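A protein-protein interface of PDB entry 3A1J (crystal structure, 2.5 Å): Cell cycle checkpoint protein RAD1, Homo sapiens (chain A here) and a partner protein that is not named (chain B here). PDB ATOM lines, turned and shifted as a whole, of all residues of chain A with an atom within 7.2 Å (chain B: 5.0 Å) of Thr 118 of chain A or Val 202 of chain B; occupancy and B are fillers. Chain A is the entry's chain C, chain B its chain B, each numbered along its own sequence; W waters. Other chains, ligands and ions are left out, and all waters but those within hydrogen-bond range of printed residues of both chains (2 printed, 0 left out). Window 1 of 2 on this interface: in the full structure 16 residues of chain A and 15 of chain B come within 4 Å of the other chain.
N of Val 119 of chain A lies within hydrogen-bond range of O of Thr 203 of chain B. The backbone carbonyl oxygen (O) of Val 117 of chain A is in hydrogen-bond range of the backbone NH (N) of His 205 of chain B (2.7 Å). OG1 of Thr 118 of chain A is in hydrogen-bond range of OG1 of Thr 204 of chain B. O of Cys 201 of chain B sits at hydrogen-bond distance from N of Lys 121 of chain A.
Of the 10 printed residues of chain B, 6 touch a printed residue of chain A. Hydrophobic or aromatic side chains of chain B within 4 Å of the printed part of chain A: Val 200, Val 202 and His 205. Of the 19 printed residues of chain A, 8 touch a printed residue of chain B.
Water W2 lies within hydrogen-bond range of O of His 205 of chain B, O of Gly 115 of chain A and N of Val 117 of chain A. Water W1 lies within hydrogen-bond range of the side-chain sulfur (SG) of Cys 201 of chain B and the side-chain amino group (NZ) of Lys 121 of chain A.
The backbone carbonyl oxygen of Leu 109 of chain A sits at hydrogen-bond distance from the backbone NH of Cys 120 of chain A (2.9 Å). The backbone carbonyl oxygen (O) of Leu 193 of chain B is in hydrogen-bond range of the backbone NH (N) of Thr 204 of chain B. The side-chain sulfur (SG) of Cys 120 of chain A lies close to the side-chain sulfur (SG) of Cys 80 of chain A, 3.6 Å away. The backbone NH (N) of Ile 195 of chain B is in hydrogen-bond range of the backbone carbonyl oxygen (O) of Val 202 of chain B, 3.0 Å away. O of Val 76 of chain A is in hydrogen-bond range of SG of Cys 80 of chain A, at 3.3 Å. N of Thr 118 of chain A sits at hydrogen-bond distance from O of Leu 111 of chain A (2.8 Å).
Asp 79 of chain A touches none of the printed residues of chain B. Of the printed residues of chain B, Thr 118 of chain A touches Val 202, Thr 203 and Thr 204. Printed residues of chain B within 4 Å of Cys 120 of chain A: Cys 201 (3.4 Å). Printed residues of chain B within 4 Å of Lys 121 of chain A: Val 200 (3.2 Å) and Cys 201 (2.8 Å). Printed residues of chain A within 4 Å of Val 200 of chain B: Val 76 (3.7 Å) and Lys 121 (3.2 Å). Of the printed residues of chain A, Val 202 of chain B touches Cys 80, Thr 118 and Val 119. Printed residues of chain A within 4 Å of Thr 203 of chain B: Val 117 (3.7 Å), Thr 118 (3.2 Å) and Val 119 (2.8 Å). The nearest residue of chain B that does not touch Thr 118 of chain A is His 205 of chain B (4.8 Å).
Among the printed residues, pairs that only touch across the chains: Lys 121 of chain A with Val 200 of chain B, Thr 118 of chain A with Thr 203 of chain B, Val 119 of chain A with Val 202 of chain B, Val 116 of chain A with His 205 of chain B, Cys 120 of chain A with Cys 201 of chain B, Val 117 of chain A with Thr 204 of chain B, Val 116 of chain A with Thr 204 of chain B, Thr 118 of chain A with Val 202 of chain B, Val 117 of chain A with Thr 203 of chain B, Val 76 of chain A with Val 200 of chain B, Cys 80 of chain A with Val 202 of chain B and Val 119 of chain A with Cys 201 of chain B.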
ATOM      1  N   VAL A  76      12.156 -22.733  25.211  1.00  0.00           N
ATOM      2  CA  VAL A  76      11.127 -23.416  24.441  1.00  0.00           C
ATOM      3  C   VAL A  76      10.547 -24.527  25.310  1.00  0.00           C
ATOM      4  O   VAL A  76       9.326 -24.696  25.400  1.00  0.00           O
ATOM      5  CB  VAL A  76      11.711 -24.042  23.160  1.00  0.00           C
ATOM      6  CG1 VAL A  76      10.698 -24.987  22.531  1.00  0.00           C
ATOM      7  CG2 VAL A  76      12.084 -22.943  22.179  1.00  0.00           C
ATOM      8  N   ASP A  79       8.286 -23.122  27.721  1.00  0.00           N
ATOM      9  CA  ASP A  79       7.106 -22.571  27.047  1.00  0.00           C
ATOM     10  C   ASP A  79       6.094 -23.680  26.770  1.00  0.00           C
ATOM     11  O   ASP A  79       4.893 -23.483  26.928  1.00  0.00           O
ATOM     12  CB  ASP A  79       7.473 -21.893  25.716  1.00  0.00           C
ATOM     13  CG  ASP A  79       7.819 -20.412  25.879  1.00  0.00           C
ATOM     14  OD1 ASP A  79       7.105 -19.717  26.644  1.00  0.00           O
ATOM     15  OD2 ASP A  79       8.790 -19.944  25.226  1.00  0.00           O
ATOM     16  N   CYS A  80       6.595 -24.838  26.349  1.00  0.00           N
ATOM     17  CA  CYS A  80       5.756 -25.986  26.047  1.00  0.00           C
ATOM     18  C   CYS A  80       5.159 -26.615  27.309  1.00  0.00           C
ATOM     19  O   CYS A  80       3.991 -27.015  27.326  1.00  0.00           O
ATOM     20  CB  CYS A  80       6.574 -27.035  25.292  1.00  0.00           C
ATOM     21  SG  CYS A  80       7.135 -26.520  23.643  1.00  0.00           S
ATOM     22  N   ILE A  83       2.148 -24.744  28.243  1.00  0.00           N
ATOM     23  CA  ILE A  83       1.330 -24.460  27.072  1.00  0.00           C
ATOM     24  C   ILE A  83      -0.135 -24.223  27.427  1.00  0.00           C
ATOM     25  O   ILE A  83      -0.842 -23.532  26.700  1.00  0.00           O
ATOM     26  CB  ILE A  83       1.408 -25.631  26.052  1.00  0.00           C
ATOM     27  CG1 ILE A  83       1.019 -25.151  24.654  1.00  0.00           C
ATOM     28  CG2 ILE A  83       0.464 -26.751  26.458  1.00  0.00           C
ATOM     29  CD1 ILE A  83       2.116 -24.368  23.954  1.00  0.00           C
ATOM     30  N   PHE A  84      -0.589 -24.788  28.543  1.00  0.00           N
ATOM     31  CA  PHE A  84      -1.988 -24.661  28.954  1.00  0.00           C
ATOM     32  C   PHE A  84      -2.305 -23.571  29.973  1.00  0.00           C
ATOM     33  O   PHE A  84      -3.411 -23.520  30.519  1.00  0.00           O
ATOM     34  CB  PHE A  84      -2.497 -26.000  29.493  1.00  0.00           C
ATOM     35  CG  PHE A  84      -2.661 -27.044  28.445  1.00  0.00           C
ATOM     36  CD1 PHE A  84      -3.478 -26.815  27.340  1.00  0.00           C
ATOM     37  CD2 PHE A  84      -2.010 -28.266  28.552  1.00  0.00           C
ATOM     38  CE1 PHE A  84      -3.645 -27.789  26.352  1.00  0.00           C
ATOM     39  CE2 PHE A  84      -2.168 -29.248  27.573  1.00  0.00           C
ATOM     40  CZ  PHE A  84      -2.990 -29.007  26.469  1.00  0.00           C
ATOM     41  N   ALA A  95      -1.111 -33.393  32.456  1.00  0.00           N
ATOM     42  CA  ALA A  95      -0.187 -34.521  32.536  1.00  0.00           C
ATOM     43  C   ALA A  95       0.890 -34.455  31.453  1.00  0.00           C
ATOM     44  O   ALA A  95       0.696 -33.849  30.405  1.00  0.00           O
ATOM     45  CB  ALA A  95      -0.955 -35.837  32.441  1.00  0.00           C
ATOM     46  N   LEU A 109       7.295 -34.043  23.663  1.00  0.00           N
ATOM     47  CA  LEU A 109       6.473 -33.782  24.826  1.00  0.00           C
ATOM     48  C   LEU A 109       5.015 -34.034  24.480  1.00  0.00           C
ATOM     49  O   LEU A 109       4.544 -33.690  23.400  1.00  0.00           O
ATOM     50  CB  LEU A 109       6.666 -32.347  25.305  1.00  0.00           C
ATOM     51  CG  LEU A 109       8.097 -31.953  25.714  1.00  0.00           C
ATOM     52  CD1 LEU A 109       8.128 -30.479  26.092  1.00  0.00           C
ATOM     53  CD2 LEU A 109       8.569 -32.792  26.884  1.00  0.00           C
ATOM     54  N   PHE A 110       4.307 -34.676  25.394  1.00  0.00           N
ATOM     55  CA  PHE A 110       2.899 -34.950  25.197  1.00  0.00           C
ATOM     56  C   PHE A 110       2.250 -34.460  26.473  1.00  0.00           C
ATOM     57  O   PHE A 110       2.514 -34.988  27.553  1.00  0.00           O
ATOM     58  CB  PHE A 110       2.655 -36.453  25.028  1.00  0.00           C
ATOM     59  CG  PHE A 110       3.438 -37.072  23.907  1.00  0.00           C
ATOM     60  CD1 PHE A 110       3.073 -36.863  22.584  1.00  0.00           C
ATOM     61  CD2 PHE A 110       4.568 -37.835  24.173  1.00  0.00           C
ATOM     62  CE1 PHE A 110       3.819 -37.402  21.543  1.00  0.00           C
ATOM     63  CE2 PHE A 110       5.327 -38.379  23.131  1.00  0.00           C
ATOM     64  CZ  PHE A 110       4.950 -38.161  21.814  1.00  0.00           C
ATOM     65  N   LEU A 111       1.415 -33.439  26.349  1.00  0.00           N
ATOM     66  CA  LEU A 111       0.728 -32.883  27.498  1.00  0.00           C
ATOM     67  C   LEU A 111      -0.769 -32.862  27.236  1.00  0.00           C
ATOM     68  O   LEU A 111      -1.206 -32.648  26.113  1.00  0.00           O
ATOM     69  CB  LEU A 111       1.217 -31.458  27.767  1.00  0.00           C
ATOM     70  CG  LEU A 111       2.728 -31.299  27.899  1.00  0.00           C
ATOM     71  CD1 LEU A 111       3.275 -30.576  26.692  1.00  0.00           C
ATOM     72  CD2 LEU A 111       3.047 -30.519  29.147  1.00  0.00           C
ATOM     73  N   GLU A 112      -1.561 -33.094  28.271  1.00  0.00           N
ATOM     74  CA  GLU A 112      -2.999 -33.055  28.091  1.00  0.00           C
ATOM     75  C   GLU A 112      -3.684 -32.435  29.297  1.00  0.00           C
ATOM     76  O   GLU A 112      -3.320 -32.684  30.451  1.00  0.00           O
ATOM     77  CB  GLU A 112      -3.550 -34.463  27.804  1.00  0.00           C
ATOM     78  CG  GLU A 112      -3.620 -35.389  29.000  1.00  0.00           C
ATOM     79  CD  GLU A 112      -4.931 -35.266  29.752  1.00  0.00           C
ATOM     80  OE1 GLU A 112      -4.939 -35.565  30.965  1.00  0.00           O
ATOM     81  OE2 GLU A 112      -5.947 -34.880  29.133  1.00  0.00           O
ATOM     82  N   GLU A 113      -4.660 -31.584  29.014  1.00  0.00           N
ATOM     83  CA  GLU A 113      -5.422 -30.924  30.057  1.00  0.00           C
ATOM     84  C   GLU A 113      -6.874 -30.941  29.623  1.00  0.00           C
ATOM     85  O   GLU A 113      -7.210 -30.475  28.538  1.00  0.00           O
ATOM     86  CB  GLU A 113      -4.967 -29.471  30.261  1.00  0.00           C
ATOM     87  CG  GLU A 113      -5.962 -28.691  31.123  1.00  0.00           C
ATOM     88  CD  GLU A 113      -5.699 -27.194  31.194  1.00  0.00           C
ATOM     89  OE1 GLU A 113      -4.753 -26.776  31.911  1.00  0.00           O
ATOM     90  OE2 GLU A 113      -6.449 -26.441  30.532  1.00  0.00           O
ATOM     91  N   GLY A 115      -8.494 -33.096  28.386  1.00  0.00           N
ATOM     92  CA  GLY A 115      -8.729 -33.798  27.139  1.00  0.00           C
ATOM     93  C   GLY A 115      -8.085 -33.161  25.923  1.00  0.00           C
ATOM     94  O   GLY A 115      -8.030 -33.776  24.852  1.00  0.00           O
ATOM     95  N   VAL A 116      -7.616 -31.924  26.066  1.00  0.00           N
ATOM     96  CA  VAL A 116      -6.949 -31.253  24.962  1.00  0.00           C
ATOM     97  C   VAL A 116      -5.517 -31.768  25.024  1.00  0.00           C
ATOM     98  O   VAL A 116      -4.935 -31.847  26.102  1.00  0.00           O
ATOM     99  CB  VAL A 116      -6.977 -29.732  25.135  1.00  0.00           C
ATOM    100  CG1 VAL A 116      -6.386 -29.063  23.912  1.00  0.00           C
ATOM    101  CG2 VAL A 116      -8.407 -29.267  25.347  1.00  0.00           C
ATOM    102  N   VAL A 117      -4.954 -32.124  23.877  1.00  0.00           N
ATOM    103  CA  VAL A 117      -3.605 -32.674  23.832  1.00  0.00           C
ATOM    104  C   VAL A 117      -2.621 -31.860  23.014  1.00  0.00           C
ATOM    105  O   VAL A 117      -2.899 -31.530  21.868  1.00  0.00           O
ATOM    106  CB  VAL A 117      -3.620 -34.080  23.226  1.00  0.00           C
ATOM    107  CG1 VAL A 117      -2.209 -34.651  23.220  1.00  0.00           C
ATOM    108  CG2 VAL A 117      -4.579 -34.969  23.998  1.00  0.00           C
ATOM    109  N   THR A 118      -1.469 -31.546  23.593  1.00  0.00           N
ATOM    110  CA  THR A 118      -0.453 -30.796  22.865  1.00  0.00           C
ATOM    111  C   THR A 118       0.758 -31.689  22.622  1.00  0.00           C
ATOM    112  O   THR A 118       1.232 -32.363  23.537  1.00  0.00           O
ATOM    113  CB  THR A 118       0.023 -29.527  23.627  1.00  0.00           C
ATOM    114  OG1 THR A 118      -1.064 -28.596  23.764  1.00  0.00           O
ATOM    115  CG2 THR A 118       1.160 -28.855  22.860  1.00  0.00           C
ATOM    116  N   VAL A 119       1.240 -31.691  21.378  1.00  0.00           N
ATOM    117  CA  VAL A 119       2.404 -32.477  20.987  1.00  0.00           C
ATOM    118  C   VAL A 119       3.528 -31.508  20.651  1.00  0.00           C
ATOM    119  O   VAL A 119       3.332 -30.586  19.869  1.00  0.00           O
ATOM    120  CB  VAL A 119       2.092 -33.354  19.761  1.00  0.00           C
ATOM    121  CG1 VAL A 119       3.321 -34.126  19.348  1.00  0.00           C
ATOM    122  CG2 VAL A 119       0.971 -34.315  20.101  1.00  0.00           C
ATOM    123  N   CYS A 120       4.698 -31.714  21.251  1.00  0.00           N
ATOM    124  CA  CYS A 120       5.844 -30.831  21.032  1.00  0.00           C
ATOM    125  C   CYS A 120       7.049 -31.613  20.540  1.00  0.00           C
ATOM    126  O   CYS A 120       7.382 -32.665  21.085  1.00  0.00           O
ATOM    127  CB  CYS A 120       6.229 -30.103  22.328  1.00  0.00           C
ATOM    128  SG  CYS A 120       4.864 -29.307  23.203  1.00  0.00           S
ATOM    129  N   LYS A 121       7.695 -31.092  19.503  1.00  0.00           N
ATOM    130  CA  LYS A 121       8.876 -31.726  18.942  1.00  0.00           C
ATOM    131  C   LYS A 121       9.997 -30.716  19.105  1.00  0.00           C
ATOM    132  O   LYS A 121      10.117 -29.764  18.331  1.00  0.00           O
ATOM    133  CB  LYS A 121       8.672 -32.050  17.460  1.00  0.00           C
ATOM    134  CG  LYS A 121       9.792 -32.893  16.880  1.00  0.00           C
ATOM    135  CD  LYS A 121       9.657 -33.066  15.374  1.00  0.00           C
ATOM    136  CE  LYS A 121      10.156 -31.843  14.621  1.00  0.00           C
ATOM    137  NZ  LYS A 121       9.857 -31.947  13.163  1.00  0.00           N
ATOM    138  N   ILE A 122      10.813 -30.929  20.124  1.00  0.00           N
ATOM    139  CA  ILE A 122      11.904 -30.026  20.415  1.00  0.00           C
ATOM    140  C   ILE A 122      13.220 -30.651  20.015  1.00  0.00           C
ATOM    141  O   ILE A 122      13.662 -31.618  20.631  1.00  0.00           O
ATOM    142  CB  ILE A 122      11.932 -29.706  21.915  1.00  0.00           C
ATOM    143  CG1 ILE A 122      10.565 -29.146  22.338  1.00  0.00           C
ATOM    144  CG2 ILE A 122      13.069 -28.746  22.216  1.00  0.00           C
ATOM    145  CD1 ILE A 122      10.366 -29.057  23.840  1.00  0.00           C
ATOM    146  N   MET B 174       2.574 -20.185  21.968  1.00  0.00           N
ATOM    147  CA  MET B 174       3.051 -20.496  20.630  1.00  0.00           C
ATOM    148  C   MET B 174       3.673 -19.257  20.007  1.00  0.00           C
ATOM    149  O   MET B 174       4.663 -19.343  19.280  1.00  0.00           O
ATOM    150  CB  MET B 174       1.910 -20.985  19.743  1.00  0.00           C
ATOM    151  CG  MET B 174       1.338 -22.322  20.152  1.00  0.00           C
ATOM    152  SD  MET B 174       0.077 -23.021  18.856  1.00  0.00           S
ATOM    153  CE  MET B 174      -1.477 -22.067  19.432  1.00  0.00           C
ATOM    154  N   LEU B 193      -4.351 -26.317  16.394  1.00  0.00           N
ATOM    155  CA  LEU B 193      -3.573 -25.098  16.298  1.00  0.00           C
ATOM    156  C   LEU B 193      -2.164 -25.647  16.085  1.00  0.00           C
ATOM    157  O   LEU B 193      -1.728 -26.552  16.799  1.00  0.00           O
ATOM    158  CB  LEU B 193      -3.668 -24.283  17.592  1.00  0.00           C
ATOM    159  CG  LEU B 193      -5.039 -23.632  17.808  1.00  0.00           C
ATOM    160  CD1 LEU B 193      -5.074 -22.864  19.120  1.00  0.00           C
ATOM    161  CD2 LEU B 193      -5.331 -22.719  16.624  1.00  0.00           C
ATOM    162  N   LYS B 194      -1.449 -25.103  15.107  1.00  0.00           N
ATOM    163  CA  LYS B 194      -0.128 -25.610  14.795  1.00  0.00           C
ATOM    164  C   LYS B 194       0.934 -24.589  14.390  1.00  0.00           C
ATOM    165  O   LYS B 194       0.676 -23.686  13.593  1.00  0.00           O
ATOM    166  CB  LYS B 194      -0.280 -26.648  13.678  1.00  0.00           C
ATOM    167  CG  LYS B 194       1.008 -27.283  13.196  1.00  0.00           C
ATOM    168  CD  LYS B 194       0.796 -28.007  11.860  1.00  0.00           C
ATOM    169  CE  LYS B 194      -0.322 -29.031  11.948  1.00  0.00           C
ATOM    170  NZ  LYS B 194      -0.502 -29.741  10.652  1.00  0.00           N
ATOM    171  N   ILE B 195       2.130 -24.738  14.949  1.00  0.00           N
ATOM    172  CA  ILE B 195       3.240 -23.875  14.587  1.00  0.00           C
ATOM    173  C   ILE B 195       4.402 -24.798  14.242  1.00  0.00           C
ATOM    174  O   ILE B 195       4.617 -25.816  14.901  1.00  0.00           O
ATOM    175  CB  ILE B 195       3.702 -22.904  15.730  1.00  0.00           C
ATOM    176  CG1 ILE B 195       4.073 -23.699  16.981  1.00  0.00           C
ATOM    177  CG2 ILE B 195       2.630 -21.852  16.009  1.00  0.00           C
ATOM    178  CD1 ILE B 195       4.813 -22.889  17.999  1.00  0.00           C
ATOM    179  N   VAL B 200      11.691 -26.332  16.422  1.00  0.00           N
ATOM    180  CA  VAL B 200      10.596 -26.780  17.280  1.00  0.00           C
ATOM    181  C   VAL B 200       9.216 -26.720  16.636  1.00  0.00           C
ATOM    182  O   VAL B 200       8.868 -25.753  15.958  1.00  0.00           O
ATOM    183  CB  VAL B 200      10.544 -25.976  18.602  1.00  0.00           C
ATOM    184  CG1 VAL B 200      10.562 -24.493  18.314  1.00  0.00           C
ATOM    185  CG2 VAL B 200       9.297 -26.343  19.391  1.00  0.00           C
ATOM    186  N   CYS B 201       8.436 -27.772  16.847  1.00  0.00           N
ATOM    187  CA  CYS B 201       7.082 -27.830  16.330  1.00  0.00           C
ATOM    188  C   CYS B 201       6.158 -28.095  17.505  1.00  0.00           C
ATOM    189  O   CYS B 201       6.525 -28.802  18.448  1.00  0.00           O
ATOM    190  CB  CYS B 201       6.925 -28.949  15.297  1.00  0.00           C
ATOM    191  SG  CYS B 201       7.853 -28.683  13.757  1.00  0.00           S
ATOM    192  N   VAL B 202       4.967 -27.512  17.452  1.00  0.00           N
ATOM    193  CA  VAL B 202       3.974 -27.683  18.500  1.00  0.00           C
ATOM    194  C   VAL B 202       2.591 -27.736  17.883  1.00  0.00           C
ATOM    195  O   VAL B 202       2.244 -26.882  17.073  1.00  0.00           O
ATOM    196  CB  VAL B 202       3.986 -26.512  19.513  1.00  0.00           C
ATOM    197  CG1 VAL B 202       2.888 -26.726  20.553  1.00  0.00           C
ATOM    198  CG2 VAL B 202       5.351 -26.393  20.171  1.00  0.00           C
ATOM    199  N   THR B 203       1.806 -28.734  18.278  1.00  0.00           N
ATOM    200  CA  THR B 203       0.441 -28.902  17.782  1.00  0.00           C
ATOM    201  C   THR B 203      -0.514 -29.188  18.926  1.00  0.00           C
ATOM    202  O   THR B 203      -0.308 -30.131  19.697  1.00  0.00           O
ATOM    203  CB  THR B 203       0.329 -30.080  16.794  1.00  0.00           C
ATOM    204  OG1 THR B 203       1.043 -29.773  15.589  1.00  0.00           O
ATOM    205  CG2 THR B 203      -1.129 -30.354  16.462  1.00  0.00           C
ATOM    206  N   THR B 204      -1.562 -28.380  19.039  1.00  0.00           N
ATOM    207  CA  THR B 204      -2.555 -28.587  20.086  1.00  0.00           C
ATOM    208  C   THR B 204      -3.836 -29.104  19.450  1.00  0.00           C
ATOM    209  O   THR B 204      -4.405 -28.465  18.560  1.00  0.00           O
ATOM    210  CB  THR B 204      -2.830 -27.288  20.867  1.00  0.00           C
ATOM    211  OG1 THR B 204      -1.672 -26.953  21.636  1.00  0.00           O
ATOM    212  CG2 THR B 204      -3.997 -27.468  21.810  1.00  0.00           C
ATOM    213  N   HIS B 205      -4.269 -30.274  19.920  1.00  0.00           N
ATOM    214  CA  HIS B 205      -5.455 -30.955  19.418  1.00  0.00           C
ATOM    215  C   HIS B 205      -6.709 -30.755  20.260  1.00  0.00           C
ATOM    216  O   HIS B 205      -6.782 -31.210  21.400  1.00  0.00           O
ATOM    217  CB  HIS B 205      -5.188 -32.462  19.336  1.00  0.00           C
ATOM    218  CG  HIS B 205      -4.024 -32.839  18.470  1.00  0.00           C
ATOM    219  ND1 HIS B 205      -4.119 -32.952  17.098  1.00  0.00           N
ATOM    220  CD2 HIS B 205      -2.746 -33.160  18.784  1.00  0.00           C
ATOM    221  CE1 HIS B 205      -2.952 -33.329  16.606  1.00  0.00           C
ATOM    222  NE2 HIS B 205      -2.101 -33.462  17.608  1.00  0.00           N
HETATM  223  O   HOH W   1      11.054 -28.961  14.176  1.00  0.00           O
HETATM  224  O   HOH W   2      -7.348 -33.867  22.050  1.00  0.00           O
